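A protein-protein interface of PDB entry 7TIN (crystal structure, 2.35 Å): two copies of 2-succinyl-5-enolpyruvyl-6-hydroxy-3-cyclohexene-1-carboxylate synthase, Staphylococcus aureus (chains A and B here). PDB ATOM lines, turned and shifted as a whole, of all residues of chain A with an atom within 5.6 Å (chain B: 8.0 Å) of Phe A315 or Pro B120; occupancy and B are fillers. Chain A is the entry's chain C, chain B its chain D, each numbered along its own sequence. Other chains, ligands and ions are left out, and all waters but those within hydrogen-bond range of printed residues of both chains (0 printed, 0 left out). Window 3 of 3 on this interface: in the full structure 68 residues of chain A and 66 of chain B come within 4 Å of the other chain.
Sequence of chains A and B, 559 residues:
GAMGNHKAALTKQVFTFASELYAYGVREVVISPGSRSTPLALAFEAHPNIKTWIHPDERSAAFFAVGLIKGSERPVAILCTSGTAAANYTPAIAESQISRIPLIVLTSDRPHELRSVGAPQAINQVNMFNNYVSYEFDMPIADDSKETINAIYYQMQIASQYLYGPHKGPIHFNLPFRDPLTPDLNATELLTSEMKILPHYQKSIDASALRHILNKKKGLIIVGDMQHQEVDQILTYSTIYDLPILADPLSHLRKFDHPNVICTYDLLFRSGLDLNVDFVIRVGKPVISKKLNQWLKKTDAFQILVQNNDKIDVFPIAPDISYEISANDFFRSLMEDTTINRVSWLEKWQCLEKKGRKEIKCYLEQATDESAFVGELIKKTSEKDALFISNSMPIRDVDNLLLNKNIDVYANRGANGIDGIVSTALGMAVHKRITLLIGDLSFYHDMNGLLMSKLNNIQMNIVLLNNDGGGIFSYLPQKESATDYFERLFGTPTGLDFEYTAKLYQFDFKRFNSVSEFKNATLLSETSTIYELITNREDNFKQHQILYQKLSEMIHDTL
Of the 13 printed residues of chain B, 6 touch a printed residue of chain A.
Printed residues of chain B that touch a printed residue of chain A: Ser B116, Gly B118, Ala B119, Pro B120, Gln B121 and Ile B123.
Hydrophobic or aromatic side chains of chain B that line the printed part of chain A: Ala B119, Pro B120 and Ile B123.
Hydrophobic or aromatic side chains of chain A within 4 Å of the printed part of chain B: Ile A98 and Phe A315.
Among the printed residues, 10 pairs touch across the chains.
No position is printed for both chains.
Of the 10 pairs that touch across the chains among the printed residues, none has its exchanged pair printed and touching as well.
Among the printed residues, pairs that only touch across the chains: Ile A98 with Gly B118 (3.5 Å), Ile A98 with Ala B119 (3.98 Å), Ile A98 with Ile B123 (3.6 Å), Asp A313 with Ala B119 (3.5 Å), Phe A315 with Pro B120 (3.8 Å), Gly A414 with Pro B120 (3.8 Å), Ala A415 with Gln B121 (3.2 Å) and Asn A416 with Pro B120 (3.8 Å).
Of chain B, only Pro B120 (3.8 Å) comes within 4 Å of Phe A315.
Pro A316 touches none of the printed residues of chain B.
Of the printed residues of chain B, Gly A414 touches Pro B120 and Gln B121.
Arg B110 touches none of the printed residues of chain A.
Of the printed residues of chain A, Ser B116 touches Asp A313 (2.4 Å).
Printed residues of chain A within 4 Å of Gly B118: Ile A98.
Of chain A, only Phe A315 (3.8 Å), Gly A414 (3.8 Å) and Asn A416 (3.8 Å) come within 4 Å of Pro B120.
The nearest residue of chain B that does not touch Phe A315 is Leu B114 (4.1 Å).
The nearest printed residue of chain B that does not touch Asn A416 is Gln B121 (4.2 Å).
The guanidinium group (NH2) of Arg A282 sits at hydrogen-bond distance from the backbone carbonyl oxygen (O) of Phe A315 (3.1 Å).
N of Phe A315 lies within hydrogen-bond range of OD2 of Asp A313 (2.9 Å).
O of Ile B123 is in hydrogen-bond range of NH1 of Arg B110, at 3.3 Å.
The backbone carbonyl oxygen (O) of Ser B82 lies within hydrogen-bond range of the side-chain amide nitrogen (NE2) of Gln B121, 2.8 Å away.
The backbone NH of Gln B121 sits at hydrogen-bond distance from the backbone carbonyl oxygen of Gly A414 (3.2 Å).
OD1 of Asp A313 is in hydrogen-bond range of OG of Ser B116 (2.4 Å).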
ATOM      1  N   ILE A  98      -7.057 -15.036 -19.756  1.00  0.00           N
ATOM      2  CA  ILE A  98      -5.966 -14.198 -19.276  1.00  0.00           C
ATOM      3  C   ILE A  98      -5.651 -14.503 -17.817  1.00  0.00           C
ATOM      4  O   ILE A  98      -4.481 -14.593 -17.429  1.00  0.00           O
ATOM      5  CB  ILE A  98      -6.304 -12.711 -19.482  1.00  0.00           C
ATOM      6  CG1 ILE A  98      -6.549 -12.425 -20.962  1.00  0.00           C
ATOM      7  CG2 ILE A  98      -5.183 -11.833 -18.954  1.00  0.00           C
ATOM      8  CD1 ILE A  98      -7.525 -11.310 -21.197  1.00  0.00           C
ATOM      9  N   ARG A 282      10.629  -9.140 -10.749  1.00  0.00           N
ATOM     10  CA  ARG A 282       9.195  -9.033 -11.003  1.00  0.00           C
ATOM     11  C   ARG A 282       8.587 -10.425 -10.872  1.00  0.00           C
ATOM     12  O   ARG A 282       8.900 -11.320 -11.662  1.00  0.00           O
ATOM     13  CB  ARG A 282       8.933  -8.445 -12.389  1.00  0.00           C
ATOM     14  CG  ARG A 282       9.525  -7.054 -12.619  1.00  0.00           C
ATOM     15  CD  ARG A 282       9.938  -6.854 -14.074  1.00  0.00           C
ATOM     16  NE  ARG A 282       8.850  -7.147 -15.000  1.00  0.00           N
ATOM     17  CZ  ARG A 282       8.927  -7.025 -16.321  1.00  0.00           C
ATOM     18  NH1 ARG A 282      10.027  -6.587 -16.915  1.00  0.00           N
ATOM     19  NH2 ARG A 282       7.876  -7.359 -17.066  1.00  0.00           N
ATOM     20  N   PRO A 286       1.325  -8.485 -13.772  1.00  0.00           N
ATOM     21  CA  PRO A 286       1.716  -7.082 -13.587  1.00  0.00           C
ATOM     22  C   PRO A 286       0.997  -6.407 -12.429  1.00  0.00           C
ATOM     23  O   PRO A 286      -0.113  -6.781 -12.045  1.00  0.00           O
ATOM     24  CB  PRO A 286       1.333  -6.431 -14.920  1.00  0.00           C
ATOM     25  CG  PRO A 286       1.389  -7.542 -15.900  1.00  0.00           C
ATOM     26  CD  PRO A 286       0.894  -8.744 -15.159  1.00  0.00           C
ATOM     27  N   ASN A 293       4.755   0.714 -13.439  1.00  0.00           N
ATOM     28  CA  ASN A 293       4.942   0.020 -14.708  1.00  0.00           C
ATOM     29  C   ASN A 293       5.687   0.895 -15.710  1.00  0.00           C
ATOM     30  O   ASN A 293       6.513   0.397 -16.485  1.00  0.00           O
ATOM     31  CB  ASN A 293       3.591  -0.420 -15.271  1.00  0.00           C
ATOM     32  CG  ASN A 293       3.132  -1.750 -14.707  1.00  0.00           C
ATOM     33  OD1 ASN A 293       3.932  -2.673 -14.533  1.00  0.00           O
ATOM     34  ND2 ASN A 293       1.839  -1.857 -14.417  1.00  0.00           N
ATOM     35  N   ASP A 313       3.399 -13.544 -20.592  1.00  0.00           N
ATOM     36  CA  ASP A 313       3.483 -12.221 -21.194  1.00  0.00           C
ATOM     37  C   ASP A 313       4.343 -11.330 -20.306  1.00  0.00           C
ATOM     38  O   ASP A 313       4.294 -11.430 -19.074  1.00  0.00           O
ATOM     39  CB  ASP A 313       2.094 -11.607 -21.388  1.00  0.00           C
ATOM     40  CG  ASP A 313       2.157 -10.160 -21.824  1.00  0.00           C
ATOM     41  OD1 ASP A 313       2.230  -9.904 -23.043  1.00  0.00           O
ATOM     42  OD2 ASP A 313       2.138  -9.278 -20.940  1.00  0.00           O
ATOM     43  N   VAL A 314       5.128 -10.455 -20.935  1.00  0.00           N
ATOM     44  CA  VAL A 314       6.185  -9.743 -20.225  1.00  0.00           C
ATOM     45  C   VAL A 314       5.849  -8.269 -20.036  1.00  0.00           C
ATOM     46  O   VAL A 314       6.751  -7.430 -19.949  1.00  0.00           O
ATOM     47  CB  VAL A 314       7.524  -9.906 -20.962  1.00  0.00           C
ATOM     48  CG1 VAL A 314       7.979 -11.351 -20.888  1.00  0.00           C
ATOM     49  CG2 VAL A 314       7.388  -9.467 -22.410  1.00  0.00           C
ATOM     50  N   PHE A 315       4.561  -7.944 -19.960  1.00  0.00           N
ATOM     51  CA  PHE A 315       4.157  -6.567 -19.697  1.00  0.00           C
ATOM     52  C   PHE A 315       4.796  -6.083 -18.395  1.00  0.00           C
ATOM     53  O   PHE A 315       4.829  -6.827 -17.406  1.00  0.00           O
ATOM     54  CB  PHE A 315       2.631  -6.468 -19.613  1.00  0.00           C
ATOM     55  CG  PHE A 315       2.110  -5.060 -19.524  1.00  0.00           C
ATOM     56  CD1 PHE A 315       1.948  -4.441 -18.292  1.00  0.00           C
ATOM     57  CD2 PHE A 315       1.777  -4.356 -20.670  1.00  0.00           C
ATOM     58  CE1 PHE A 315       1.475  -3.145 -18.208  1.00  0.00           C
ATOM     59  CE2 PHE A 315       1.297  -3.060 -20.595  1.00  0.00           C
ATOM     60  CZ  PHE A 315       1.146  -2.454 -19.361  1.00  0.00           C
ATOM     61  N   PRO A 316       5.311  -4.842 -18.350  1.00  0.00           N
ATOM     62  CA  PRO A 316       5.282  -3.805 -19.387  1.00  0.00           C
ATOM     63  C   PRO A 316       6.475  -3.785 -20.348  1.00  0.00           C
ATOM     64  O   PRO A 316       6.471  -2.984 -21.283  1.00  0.00           O
ATOM     65  CB  PRO A 316       5.272  -2.523 -18.562  1.00  0.00           C
ATOM     66  CG  PRO A 316       6.161  -2.861 -17.415  1.00  0.00           C
ATOM     67  CD  PRO A 316       5.888  -4.322 -17.097  1.00  0.00           C
ATOM     68  N   ILE A 317       7.483  -4.627 -20.126  1.00  0.00           N
ATOM     69  CA  ILE A 317       8.681  -4.597 -20.957  1.00  0.00           C
ATOM     70  C   ILE A 317       9.411  -5.923 -20.812  1.00  0.00           C
ATOM     71  O   ILE A 317       9.378  -6.557 -19.755  1.00  0.00           O
ATOM     72  CB  ILE A 317       9.587  -3.394 -20.586  1.00  0.00           C
ATOM     73  CG1 ILE A 317      10.556  -3.087 -21.727  1.00  0.00           C
ATOM     74  CG2 ILE A 317      10.334  -3.650 -19.278  1.00  0.00           C
ATOM     75  CD1 ILE A 317      11.515  -1.965 -21.424  1.00  0.00           C
ATOM     76  N   GLY A 414      -7.714  -9.770 -14.971  1.00  0.00           N
ATOM     77  CA  GLY A 414      -7.174 -10.382 -16.168  1.00  0.00           C
ATOM     78  C   GLY A 414      -7.483  -9.566 -17.404  1.00  0.00           C
ATOM     79  O   GLY A 414      -6.599  -8.911 -17.963  1.00  0.00           O
ATOM     80  N   ALA A 415      -8.738  -9.601 -17.845  1.00  0.00           N
ATOM     81  CA  ALA A 415      -9.174  -8.752 -18.945  1.00  0.00           C
ATOM     82  C   ALA A 415      -9.577  -7.357 -18.486  1.00  0.00           C
ATOM     83  O   ALA A 415      -9.848  -6.502 -19.334  1.00  0.00           O
ATOM     84  CB  ALA A 415     -10.339  -9.409 -19.690  1.00  0.00           C
ATOM     85  N   ASN A 416      -9.637  -7.122 -17.172  1.00  0.00           N
ATOM     86  CA  ASN A 416      -9.936  -5.811 -16.593  1.00  0.00           C
ATOM     87  C   ASN A 416     -11.302  -5.283 -17.028  1.00  0.00           C
ATOM     88  O   ASN A 416     -11.522  -4.073 -17.089  1.00  0.00           O
ATOM     89  CB  ASN A 416      -8.835  -4.795 -16.920  1.00  0.00           C
ATOM     90  CG  ASN A 416      -7.486  -5.202 -16.357  1.00  0.00           C
ATOM     91  OD1 ASN A 416      -7.383  -6.176 -15.611  1.00  0.00           O
ATOM     92  ND2 ASN A 416      -6.447  -4.462 -16.711  1.00  0.00           N
ATOM     93  N   SER B  82     -11.307  -1.875 -26.290  1.00  0.00           N
ATOM     94  CA  SER B  82     -10.616  -3.154 -26.356  1.00  0.00           C
ATOM     95  C   SER B  82     -10.956  -4.027 -25.149  1.00  0.00           C
ATOM     96  O   SER B  82     -11.288  -3.533 -24.069  1.00  0.00           O
ATOM     97  CB  SER B  82      -9.105  -2.931 -26.441  1.00  0.00           C
ATOM     98  OG  SER B  82      -8.549  -2.720 -25.157  1.00  0.00           O
ATOM     99  N   GLY B  83     -10.892  -5.343 -25.352  1.00  0.00           N
ATOM    100  CA  GLY B  83     -11.072  -6.284 -24.259  1.00  0.00           C
ATOM    101  C   GLY B  83     -12.364  -7.079 -24.269  1.00  0.00           C
ATOM    102  O   GLY B  83     -12.888  -7.420 -25.336  1.00  0.00           O
ATOM    103  N   ARG B 110      -5.536  -2.125 -29.231  1.00  0.00           N
ATOM    104  CA  ARG B 110      -4.224  -1.563 -28.973  1.00  0.00           C
ATOM    105  C   ARG B 110      -3.371  -1.655 -30.238  1.00  0.00           C
ATOM    106  O   ARG B 110      -3.586  -2.537 -31.075  1.00  0.00           O
ATOM    107  CB  ARG B 110      -3.541  -2.306 -27.822  1.00  0.00           C
ATOM    108  CG  ARG B 110      -4.404  -2.490 -26.574  1.00  0.00           C
ATOM    109  CD  ARG B 110      -5.162  -3.823 -26.577  1.00  0.00           C
ATOM    110  NE  ARG B 110      -4.292  -4.979 -26.776  1.00  0.00           N
ATOM    111  CZ  ARG B 110      -4.676  -6.115 -27.343  1.00  0.00           C
ATOM    112  NH1 ARG B 110      -5.908  -6.281 -27.795  1.00  0.00           N
ATOM    113  NH2 ARG B 110      -3.802  -7.110 -27.461  1.00  0.00           N
ATOM    114  N   GLU B 113       2.440  -2.620 -31.369  1.00  0.00           N
ATOM    115  CA  GLU B 113       3.537  -2.705 -30.412  1.00  0.00           C
ATOM    116  C   GLU B 113       3.065  -3.180 -29.047  1.00  0.00           C
ATOM    117  O   GLU B 113       3.855  -3.748 -28.284  1.00  0.00           O
ATOM    118  CB  GLU B 113       4.227  -1.347 -30.276  1.00  0.00           C
ATOM    119  CG  GLU B 113       3.356  -0.271 -29.644  1.00  0.00           C
ATOM    120  CD  GLU B 113       2.770   0.670 -30.677  1.00  0.00           C
ATOM    121  OE1 GLU B 113       2.487   0.212 -31.807  1.00  0.00           O
ATOM    122  OE2 GLU B 113       2.592   1.867 -30.362  1.00  0.00           O
ATOM    123  N   LEU B 114       1.795  -2.960 -28.717  1.00  0.00           N
ATOM    124  CA  LEU B 114       1.287  -3.296 -27.397  1.00  0.00           C
ATOM    125  C   LEU B 114       0.330  -4.477 -27.394  1.00  0.00           C
ATOM    126  O   LEU B 114      -0.082  -4.909 -26.310  1.00  0.00           O
ATOM    127  CB  LEU B 114       0.591  -2.077 -26.770  1.00  0.00           C
ATOM    128  CG  LEU B 114       1.427  -1.260 -25.777  1.00  0.00           C
ATOM    129  CD1 LEU B 114       0.656  -0.041 -25.300  1.00  0.00           C
ATOM    130  CD2 LEU B 114       1.876  -2.111 -24.591  1.00  0.00           C
ATOM    131  N   SER B 116      -0.650  -8.118 -27.238  1.00  0.00           N
ATOM    132  CA  SER B 116       0.002  -9.343 -26.799  1.00  0.00           C
ATOM    133  C   SER B 116      -1.041 -10.125 -26.017  1.00  0.00           C
ATOM    134  O   SER B 116      -1.479  -9.674 -24.956  1.00  0.00           O
ATOM    135  CB  SER B 116       1.230  -9.035 -25.949  1.00  0.00           C
ATOM    136  OG  SER B 116       1.780 -10.219 -25.395  1.00  0.00           O
ATOM    137  N   VAL B 117      -1.453 -11.272 -26.555  1.00  0.00           N
ATOM    138  CA  VAL B 117      -2.484 -12.075 -25.907  1.00  0.00           C
ATOM    139  C   VAL B 117      -1.981 -12.520 -24.540  1.00  0.00           C
ATOM    140  O   VAL B 117      -0.944 -13.184 -24.427  1.00  0.00           O
ATOM    141  CB  VAL B 117      -2.871 -13.262 -26.794  1.00  0.00           C
ATOM    142  CG1 VAL B 117      -4.126 -13.937 -26.265  1.00  0.00           C
ATOM    143  CG2 VAL B 117      -3.081 -12.785 -28.227  1.00  0.00           C
ATOM    144  N   GLY B 118      -2.710 -12.140 -23.490  1.00  0.00           N
ATOM    145  CA  GLY B 118      -2.329 -12.411 -22.121  1.00  0.00           C
ATOM    146  C   GLY B 118      -1.914 -11.185 -21.334  1.00  0.00           C
ATOM    147  O   GLY B 118      -1.921 -11.230 -20.099  1.00  0.00           O
ATOM    148  N   ALA B 119      -1.538 -10.100 -22.011  1.00  0.00           N
ATOM    149  CA  ALA B 119      -1.274  -8.828 -21.353  1.00  0.00           C
ATOM    150  C   ALA B 119      -2.576  -8.297 -20.750  1.00  0.00           C
ATOM    151  O   ALA B 119      -3.657  -8.814 -21.042  1.00  0.00           O
ATOM    152  CB  ALA B 119      -0.673  -7.840 -22.355  1.00  0.00           C
ATOM    153  N   PRO B 120      -2.509  -7.279 -19.886  1.00  0.00           N
ATOM    154  CA  PRO B 120      -3.746  -6.753 -19.284  1.00  0.00           C
ATOM    155  C   PRO B 120      -4.724  -6.257 -20.340  1.00  0.00           C
ATOM    156  O   PRO B 120      -4.371  -5.448 -21.203  1.00  0.00           O
ATOM    157  CB  PRO B 120      -3.248  -5.606 -18.396  1.00  0.00           C
ATOM    158  CG  PRO B 120      -1.843  -5.957 -18.080  1.00  0.00           C
ATOM    159  CD  PRO B 120      -1.309  -6.653 -19.297  1.00  0.00           C
ATOM    160  N   GLN B 121      -5.963  -6.762 -20.269  1.00  0.00           N
ATOM    161  CA  GLN B 121      -7.057  -6.336 -21.151  1.00  0.00           C
ATOM    162  C   GLN B 121      -6.746  -6.627 -22.620  1.00  0.00           C
ATOM    163  O   GLN B 121      -7.177  -5.898 -23.517  1.00  0.00           O
ATOM    164  CB  GLN B 121      -7.375  -4.847 -20.948  1.00  0.00           C
ATOM    165  CG  GLN B 121      -8.749  -4.382 -21.423  1.00  0.00           C
ATOM    166  CD  GLN B 121      -8.966  -2.902 -21.173  1.00  0.00           C
ATOM    167  OE1 GLN B 121      -8.365  -2.323 -20.268  1.00  0.00           O
ATOM    168  NE2 GLN B 121      -9.818  -2.277 -21.984  1.00  0.00           N
ATOM    169  N   ALA B 122      -6.004  -7.703 -22.884  1.00  0.00           N
ATOM    170  CA  ALA B 122      -5.494  -8.000 -24.223  1.00  0.00           C
ATOM    171  C   ALA B 122      -5.865  -9.426 -24.628  1.00  0.00           C
ATOM    172  O   ALA B 122      -5.098 -10.368 -24.408  1.00  0.00           O
ATOM    173  CB  ALA B 122      -3.985  -7.779 -24.275  1.00  0.00           C
ATOM    174  N   ILE B 123      -7.045  -9.582 -25.216  1.00  0.00           N
ATOM    175  CA  ILE B 123      -7.379 -10.790 -25.955  1.00  0.00           C
ATOM    176  C   ILE B 123      -7.056 -10.535 -27.419  1.00  0.00           C
ATOM    177  O   ILE B 123      -6.932  -9.391 -27.857  1.00  0.00           O
ATOM    178  CB  ILE B 123      -8.858 -11.200 -25.783  1.00  0.00           C
ATOM    179  CG1 ILE B 123      -9.778 -10.023 -26.113  1.00  0.00           C
ATOM    180  CG2 ILE B 123      -9.123 -11.704 -24.380  1.00  0.00           C
ATOM    181  CD1 ILE B 123     -11.098 -10.430 -26.705  1.00  0.00           C
